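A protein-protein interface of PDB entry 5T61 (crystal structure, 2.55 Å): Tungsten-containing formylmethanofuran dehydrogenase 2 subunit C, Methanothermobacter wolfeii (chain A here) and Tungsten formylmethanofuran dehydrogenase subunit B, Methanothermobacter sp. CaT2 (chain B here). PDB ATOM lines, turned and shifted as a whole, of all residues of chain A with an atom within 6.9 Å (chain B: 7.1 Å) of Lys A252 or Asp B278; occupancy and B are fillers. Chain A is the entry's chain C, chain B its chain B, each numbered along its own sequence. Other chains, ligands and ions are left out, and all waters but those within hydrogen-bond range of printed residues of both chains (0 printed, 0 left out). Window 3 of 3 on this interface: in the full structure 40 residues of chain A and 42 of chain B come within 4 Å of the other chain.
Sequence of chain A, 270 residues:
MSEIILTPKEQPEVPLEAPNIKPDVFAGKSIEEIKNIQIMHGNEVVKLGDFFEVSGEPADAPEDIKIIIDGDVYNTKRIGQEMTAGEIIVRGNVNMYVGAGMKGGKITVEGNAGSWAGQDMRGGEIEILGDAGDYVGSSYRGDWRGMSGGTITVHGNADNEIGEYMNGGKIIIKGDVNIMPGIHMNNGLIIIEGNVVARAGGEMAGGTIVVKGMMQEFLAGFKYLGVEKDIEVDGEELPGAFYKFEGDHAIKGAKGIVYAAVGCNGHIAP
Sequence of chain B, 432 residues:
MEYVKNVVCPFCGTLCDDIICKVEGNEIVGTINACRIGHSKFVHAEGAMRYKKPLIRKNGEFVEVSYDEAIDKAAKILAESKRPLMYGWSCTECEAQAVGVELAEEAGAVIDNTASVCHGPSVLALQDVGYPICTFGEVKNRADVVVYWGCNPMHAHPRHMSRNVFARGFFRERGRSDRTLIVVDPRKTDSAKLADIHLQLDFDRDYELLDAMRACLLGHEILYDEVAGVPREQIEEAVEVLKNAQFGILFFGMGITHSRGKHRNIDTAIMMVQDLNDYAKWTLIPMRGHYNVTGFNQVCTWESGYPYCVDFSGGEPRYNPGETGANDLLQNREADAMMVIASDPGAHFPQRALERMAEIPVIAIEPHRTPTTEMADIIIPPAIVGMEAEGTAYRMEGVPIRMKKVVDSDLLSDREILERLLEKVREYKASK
NH2 of Arg B214 is in hydrogen-bond range of O of Ala A250 (3.0 Å).
OD1 of Asp B275 lies within salt-bridge range of NZ of Lys A252 (3.8 Å).
The side-chain amino group of Lys A252 is in salt-bridge range of the side-chain carboxylate of Asp B278 (3.1 Å).
NH2 of Arg B214 sits close to SD of Met B271 (3.8 Å).
O of Leu B218 lies close to ND1 of His B220, at 3.5 Å.
The backbone NH (N) of Ala A250 lies close to the side-chain carboxylate (OD1) of Asp A248 (3.2 Å).
Among the printed residues, merely in contact across the chains: Ala A250 with Leu B218, His A249 with Leu B218, His A249 with His B220, Ile A251 with Arg B214, Ile A251 with Met B271 and Lys A252 with Leu B218.
Of the printed residues of chain B, Ala A250 touches Arg B214 and Leu B218.
Lys A252 touches just these residues of chain B: Leu B218 (3.7 Å), Asp B275 (3.8 Å) and Asp B278 (3.1 Å).
Gly A253 touches none of the printed residues of chain B.
Lys A255 touches none of the printed residues of chain B.
Of the printed residues of chain A, Asp B275 touches Lys A252.
The nearest residue of chain B that does not touch Lys A252 is Arg B214 (6.2 Å).
Hydrophobic or aromatic side chains of chain B that line the printed part of chain A: Leu B218, His B220 and Met B271.
Hydrophobic or aromatic side chains of chain A that line the printed part of chain B: His A249, Ala A250 and Ile A251.
Among the printed residues, 9 pairs touch across the chains.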
ATOM      1  N   ALA A 205      20.921  28.278  12.720  1.00  0.00           N
ATOM      2  CA  ALA A 205      19.949  29.154  12.082  1.00  0.00           C
ATOM      3  C   ALA A 205      19.645  30.394  12.905  1.00  0.00           C
ATOM      4  O   ALA A 205      19.248  31.420  12.344  1.00  0.00           O
ATOM      5  CB  ALA A 205      18.647  28.395  11.808  1.00  0.00           C
ATOM      6  N   ASP A 248      24.798  30.359  10.347  1.00  0.00           N
ATOM      7  CA  ASP A 248      25.679  29.802   9.327  1.00  0.00           C
ATOM      8  C   ASP A 248      24.971  29.868   7.972  1.00  0.00           C
ATOM      9  O   ASP A 248      23.928  29.245   7.781  1.00  0.00           O
ATOM     10  CB  ASP A 248      26.054  28.360   9.701  1.00  0.00           C
ATOM     11  CG  ASP A 248      27.004  27.703   8.710  1.00  0.00           C
ATOM     12  OD1 ASP A 248      27.395  28.339   7.707  1.00  0.00           O
ATOM     13  OD2 ASP A 248      27.364  26.532   8.947  1.00  0.00           O
ATOM     14  N   HIS A 249      25.531  30.630   7.034  1.00  0.00           N
ATOM     15  CA  HIS A 249      24.840  30.894   5.778  1.00  0.00           C
ATOM     16  C   HIS A 249      24.843  29.713   4.814  1.00  0.00           C
ATOM     17  O   HIS A 249      24.337  29.854   3.696  1.00  0.00           O
ATOM     18  CB  HIS A 249      25.435  32.129   5.098  1.00  0.00           C
ATOM     19  CG  HIS A 249      25.067  33.413   5.771  1.00  0.00           C
ATOM     20  ND1 HIS A 249      25.993  34.231   6.382  1.00  0.00           N
ATOM     21  CD2 HIS A 249      23.864  34.012   5.943  1.00  0.00           C
ATOM     22  CE1 HIS A 249      25.378  35.282   6.893  1.00  0.00           C
ATOM     23  NE2 HIS A 249      24.085  35.173   6.642  1.00  0.00           N
ATOM     24  N   ALA A 250      25.374  28.555   5.212  1.00  0.00           N
ATOM     25  CA  ALA A 250      25.014  27.323   4.521  1.00  0.00           C
ATOM     26  C   ALA A 250      23.543  26.985   4.725  1.00  0.00           C
ATOM     27  O   ALA A 250      22.993  26.166   3.980  1.00  0.00           O
ATOM     28  CB  ALA A 250      25.891  26.166   4.994  1.00  0.00           C
ATOM     29  N   ILE A 251      22.908  27.595   5.728  1.00  0.00           N
ATOM     30  CA  ILE A 251      21.490  27.426   6.024  1.00  0.00           C
ATOM     31  C   ILE A 251      20.742  28.633   5.477  1.00  0.00           C
ATOM     32  O   ILE A 251      21.225  29.769   5.564  1.00  0.00           O
ATOM     33  CB  ILE A 251      21.260  27.270   7.541  1.00  0.00           C
ATOM     34  CG1 ILE A 251      21.964  26.019   8.070  1.00  0.00           C
ATOM     35  CG2 ILE A 251      19.775  27.242   7.871  1.00  0.00           C
ATOM     36  CD1 ILE A 251      21.324  24.734   7.631  1.00  0.00           C
ATOM     37  N   LYS A 252      19.562  28.394   4.914  1.00  0.00           N
ATOM     38  CA  LYS A 252      18.756  29.482   4.374  1.00  0.00           C
ATOM     39  C   LYS A 252      18.185  30.341   5.496  1.00  0.00           C
ATOM     40  O   LYS A 252      17.705  29.830   6.512  1.00  0.00           O
ATOM     41  CB  LYS A 252      17.628  28.928   3.504  1.00  0.00           C
ATOM     42  CG  LYS A 252      18.083  28.486   2.119  1.00  0.00           C
ATOM     43  CD  LYS A 252      17.056  27.598   1.428  1.00  0.00           C
ATOM     44  CE  LYS A 252      17.624  27.021   0.137  1.00  0.00           C
ATOM     45  NZ  LYS A 252      16.711  26.044  -0.518  1.00  0.00           N
ATOM     46  N   GLY A 253      18.250  31.658   5.309  1.00  0.00           N
ATOM     47  CA  GLY A 253      17.692  32.590   6.273  1.00  0.00           C
ATOM     48  C   GLY A 253      18.389  32.626   7.614  1.00  0.00           C
ATOM     49  O   GLY A 253      17.769  32.996   8.613  1.00  0.00           O
ATOM     50  N   ALA A 254      19.669  32.267   7.662  1.00  0.00           N
ATOM     51  CA  ALA A 254      20.369  32.125   8.932  1.00  0.00           C
ATOM     52  C   ALA A 254      20.578  33.478   9.605  1.00  0.00           C
ATOM     53  O   ALA A 254      21.003  34.445   8.965  1.00  0.00           O
ATOM     54  CB  ALA A 254      21.714  31.434   8.717  1.00  0.00           C
ATOM     55  N   LYS A 255      20.279  33.539  10.910  1.00  0.00           N
ATOM     56  CA  LYS A 255      20.463  34.744  11.711  1.00  0.00           C
ATOM     57  C   LYS A 255      21.273  34.481  12.977  1.00  0.00           C
ATOM     58  O   LYS A 255      21.199  35.270  13.924  1.00  0.00           O
ATOM     59  CB  LYS A 255      19.118  35.366  12.091  1.00  0.00           C
ATOM     60  CG  LYS A 255      18.235  35.768  10.927  1.00  0.00           C
ATOM     61  CD  LYS A 255      18.747  37.054  10.300  1.00  0.00           C
ATOM     62  CE  LYS A 255      17.910  37.463   9.105  1.00  0.00           C
ATOM     63  NZ  LYS A 255      18.295  38.814   8.615  1.00  0.00           N
ATOM     64  N   ARG B 214      28.349  25.221   0.333  1.00  0.00           N
ATOM     65  CA  ARG B 214      26.923  25.520   0.470  1.00  0.00           C
ATOM     66  C   ARG B 214      26.664  27.015   0.609  1.00  0.00           C
ATOM     67  O   ARG B 214      25.665  27.523   0.087  1.00  0.00           O
ATOM     68  CB  ARG B 214      26.327  24.765   1.655  1.00  0.00           C
ATOM     69  CG  ARG B 214      26.353  23.260   1.532  1.00  0.00           C
ATOM     70  CD  ARG B 214      26.004  22.615   2.856  1.00  0.00           C
ATOM     71  NE  ARG B 214      24.768  23.158   3.411  1.00  0.00           N
ATOM     72  CZ  ARG B 214      24.273  22.818   4.597  1.00  0.00           C
ATOM     73  NH1 ARG B 214      24.906  21.926   5.346  1.00  0.00           N
ATOM     74  NH2 ARG B 214      23.147  23.370   5.035  1.00  0.00           N
ATOM     75  N   LEU B 218      24.301  29.143  -2.047  1.00  0.00           N
ATOM     76  CA  LEU B 218      23.181  30.021  -1.739  1.00  0.00           C
ATOM     77  C   LEU B 218      23.501  31.494  -1.971  1.00  0.00           C
ATOM     78  O   LEU B 218      22.755  32.358  -1.496  1.00  0.00           O
ATOM     79  CB  LEU B 218      22.725  29.818  -0.290  1.00  0.00           C
ATOM     80  CG  LEU B 218      22.379  28.399   0.171  1.00  0.00           C
ATOM     81  CD1 LEU B 218      22.196  28.362   1.683  1.00  0.00           C
ATOM     82  CD2 LEU B 218      21.142  27.867  -0.544  1.00  0.00           C
ATOM     83  N   HIS B 220      26.333  33.362  -1.185  1.00  0.00           N
ATOM     84  CA  HIS B 220      27.134  34.093  -0.215  1.00  0.00           C
ATOM     85  C   HIS B 220      28.611  34.039  -0.565  1.00  0.00           C
ATOM     86  O   HIS B 220      29.060  33.218  -1.370  1.00  0.00           O
ATOM     87  CB  HIS B 220      26.906  33.552   1.194  1.00  0.00           C
ATOM     88  CG  HIS B 220      25.526  33.806   1.712  1.00  0.00           C
ATOM     89  ND1 HIS B 220      24.476  32.939   1.496  1.00  0.00           N
ATOM     90  CD2 HIS B 220      25.022  34.835   2.433  1.00  0.00           C
ATOM     91  CE1 HIS B 220      23.386  33.423   2.063  1.00  0.00           C
ATOM     92  NE2 HIS B 220      23.690  34.572   2.638  1.00  0.00           N
ATOM     93  N   MET B 271      22.438  18.024   3.068  1.00  0.00           N
ATOM     94  CA  MET B 271      21.716  19.282   2.918  1.00  0.00           C
ATOM     95  C   MET B 271      22.174  20.048   1.682  1.00  0.00           C
ATOM     96  O   MET B 271      21.390  20.810   1.105  1.00  0.00           O
ATOM     97  CB  MET B 271      21.870  20.141   4.173  1.00  0.00           C
ATOM     98  CG  MET B 271      21.189  19.571   5.415  1.00  0.00           C
ATOM     99  SD  MET B 271      21.083  20.763   6.771  1.00  0.00           S
ATOM    100  CE  MET B 271      19.763  21.817   6.178  1.00  0.00           C
ATOM    101  N   VAL B 273      23.129  18.479  -1.207  1.00  0.00           N
ATOM    102  CA  VAL B 273      22.438  17.754  -2.271  1.00  0.00           C
ATOM    103  C   VAL B 273      20.977  18.181  -2.348  1.00  0.00           C
ATOM    104  O   VAL B 273      20.426  18.369  -3.441  1.00  0.00           O
ATOM    105  CB  VAL B 273      22.586  16.236  -2.056  1.00  0.00           C
ATOM    106  CG1 VAL B 273      21.617  15.467  -2.943  1.00  0.00           C
ATOM    107  CG2 VAL B 273      24.020  15.805  -2.325  1.00  0.00           C
ATOM    108  N   GLN B 274      20.326  18.327  -1.194  1.00  0.00           N
ATOM    109  CA  GLN B 274      18.947  18.803  -1.173  1.00  0.00           C
ATOM    110  C   GLN B 274      18.824  20.183  -1.812  1.00  0.00           C
ATOM    111  O   GLN B 274      18.017  20.387  -2.727  1.00  0.00           O
ATOM    112  CB  GLN B 274      18.426  18.833   0.262  1.00  0.00           C
ATOM    113  CG  GLN B 274      18.166  17.468   0.862  1.00  0.00           C
ATOM    114  CD  GLN B 274      17.809  17.548   2.332  1.00  0.00           C
ATOM    115  OE1 GLN B 274      18.048  18.564   2.984  1.00  0.00           O
ATOM    116  NE2 GLN B 274      17.222  16.479   2.859  1.00  0.00           N
ATOM    117  N   ASP B 275      19.623  21.145  -1.341  1.00  0.00           N
ATOM    118  CA  ASP B 275      19.500  22.523  -1.812  1.00  0.00           C
ATOM    119  C   ASP B 275      19.869  22.666  -3.282  1.00  0.00           C
ATOM    120  O   ASP B 275      19.336  23.545  -3.970  1.00  0.00           O
ATOM    121  CB  ASP B 275      20.375  23.441  -0.960  1.00  0.00           C
ATOM    122  CG  ASP B 275      19.861  23.576   0.458  1.00  0.00           C
ATOM    123  OD1 ASP B 275      18.767  23.043   0.742  1.00  0.00           O
ATOM    124  OD2 ASP B 275      20.547  24.207   1.289  1.00  0.00           O
ATOM    125  N   LEU B 276      20.771  21.816  -3.776  1.00  0.00           N
ATOM    126  CA  LEU B 276      21.144  21.841  -5.185  1.00  0.00           C
ATOM    127  C   LEU B 276      19.958  21.587  -6.104  1.00  0.00           C
ATOM    128  O   LEU B 276      19.996  21.986  -7.273  1.00  0.00           O
ATOM    129  CB  LEU B 276      22.255  20.817  -5.434  1.00  0.00           C
ATOM    130  CG  LEU B 276      23.666  21.332  -5.150  1.00  0.00           C
ATOM    131  CD1 LEU B 276      24.603  20.195  -4.812  1.00  0.00           C
ATOM    132  CD2 LEU B 276      24.160  22.053  -6.392  1.00  0.00           C
ATOM    133  N   ASN B 277      18.897  20.957  -5.599  1.00  0.00           N
ATOM    134  CA  ASN B 277      17.746  20.648  -6.435  1.00  0.00           C
ATOM    135  C   ASN B 277      16.977  21.889  -6.867  1.00  0.00           C
ATOM    136  O   ASN B 277      16.067  21.770  -7.694  1.00  0.00           O
ATOM    137  CB  ASN B 277      16.819  19.669  -5.712  1.00  0.00           C
ATOM    138  CG  ASN B 277      17.356  18.248  -5.721  1.00  0.00           C
ATOM    139  OD1 ASN B 277      16.980  17.440  -6.569  1.00  0.00           O
ATOM    140  ND2 ASN B 277      18.236  17.936  -4.773  1.00  0.00           N
ATOM    141  N   ASP B 278      17.308  23.068  -6.332  1.00  0.00           N
ATOM    142  CA  ASP B 278      16.769  24.310  -6.877  1.00  0.00           C
ATOM    143  C   ASP B 278      17.462  24.731  -8.167  1.00  0.00           C
ATOM    144  O   ASP B 278      16.913  25.552  -8.909  1.00  0.00           O
ATOM    145  CB  ASP B 278      16.888  25.444  -5.857  1.00  0.00           C
ATOM    146  CG  ASP B 278      15.849  25.359  -4.758  1.00  0.00           C
ATOM    147  OD1 ASP B 278      14.687  25.029  -5.065  1.00  0.00           O
ATOM    148  OD2 ASP B 278      16.191  25.647  -3.588  1.00  0.00           O
ATOM    149  N   TYR B 279      18.643  24.184  -8.451  1.00  0.00           N
ATOM    150  CA  TYR B 279      19.388  24.464  -9.672  1.00  0.00           C
ATOM    151  C   TYR B 279      19.552  23.262 -10.585  1.00  0.00           C
ATOM    152  O   TYR B 279      19.683  23.441 -11.797  1.00  0.00           O
ATOM    153  CB  TYR B 279      20.784  25.002  -9.325  1.00  0.00           C
ATOM    154  CG  TYR B 279      20.763  26.277  -8.521  1.00  0.00           C
ATOM    155  CD1 TYR B 279      20.584  27.504  -9.143  1.00  0.00           C
ATOM    156  CD2 TYR B 279      20.864  26.250  -7.137  1.00  0.00           C
ATOM    157  CE1 TYR B 279      20.554  28.676  -8.414  1.00  0.00           C
ATOM    158  CE2 TYR B 279      20.826  27.414  -6.397  1.00  0.00           C
ATOM    159  CZ  TYR B 279      20.670  28.625  -7.040  1.00  0.00           C
ATOM    160  OH  TYR B 279      20.632  29.789  -6.307  1.00  0.00           O
ATOM    161  N   ALA B 280      19.569  22.053 -10.038  1.00  0.00           N
ATOM    162  CA  ALA B 280      19.808  20.864 -10.833  1.00  0.00           C
ATOM    163  C   ALA B 280      19.347  19.656 -10.042  1.00  0.00           C
ATOM    164  O   ALA B 280      19.435  19.638  -8.813  1.00  0.00           O
ATOM    165  CB  ALA B 280      21.289  20.717 -11.193  1.00  0.00           C
ATOM    166  N   LYS B 281      18.863  18.647 -10.757  1.00  0.00           N
ATOM    167  CA  LYS B 281      18.448  17.424 -10.086  1.00  0.00           C
ATOM    168  C   LYS B 281      19.655  16.799  -9.411  1.00  0.00           C
ATOM    169  O   LYS B 281      20.700  16.607 -10.040  1.00  0.00           O
ATOM    170  CB  LYS B 281      17.840  16.449 -11.088  1.00  0.00           C
ATOM    171  CG  LYS B 281      16.621  15.713 -10.573  1.00  0.00           C
ATOM    172  CD  LYS B 281      16.951  14.341 -10.033  1.00  0.00           C
ATOM    173  CE  LYS B 281      16.254  14.121  -8.702  1.00  0.00           C
ATOM    174  NZ  LYS B 281      15.089  13.200  -8.800  1.00  0.00           N
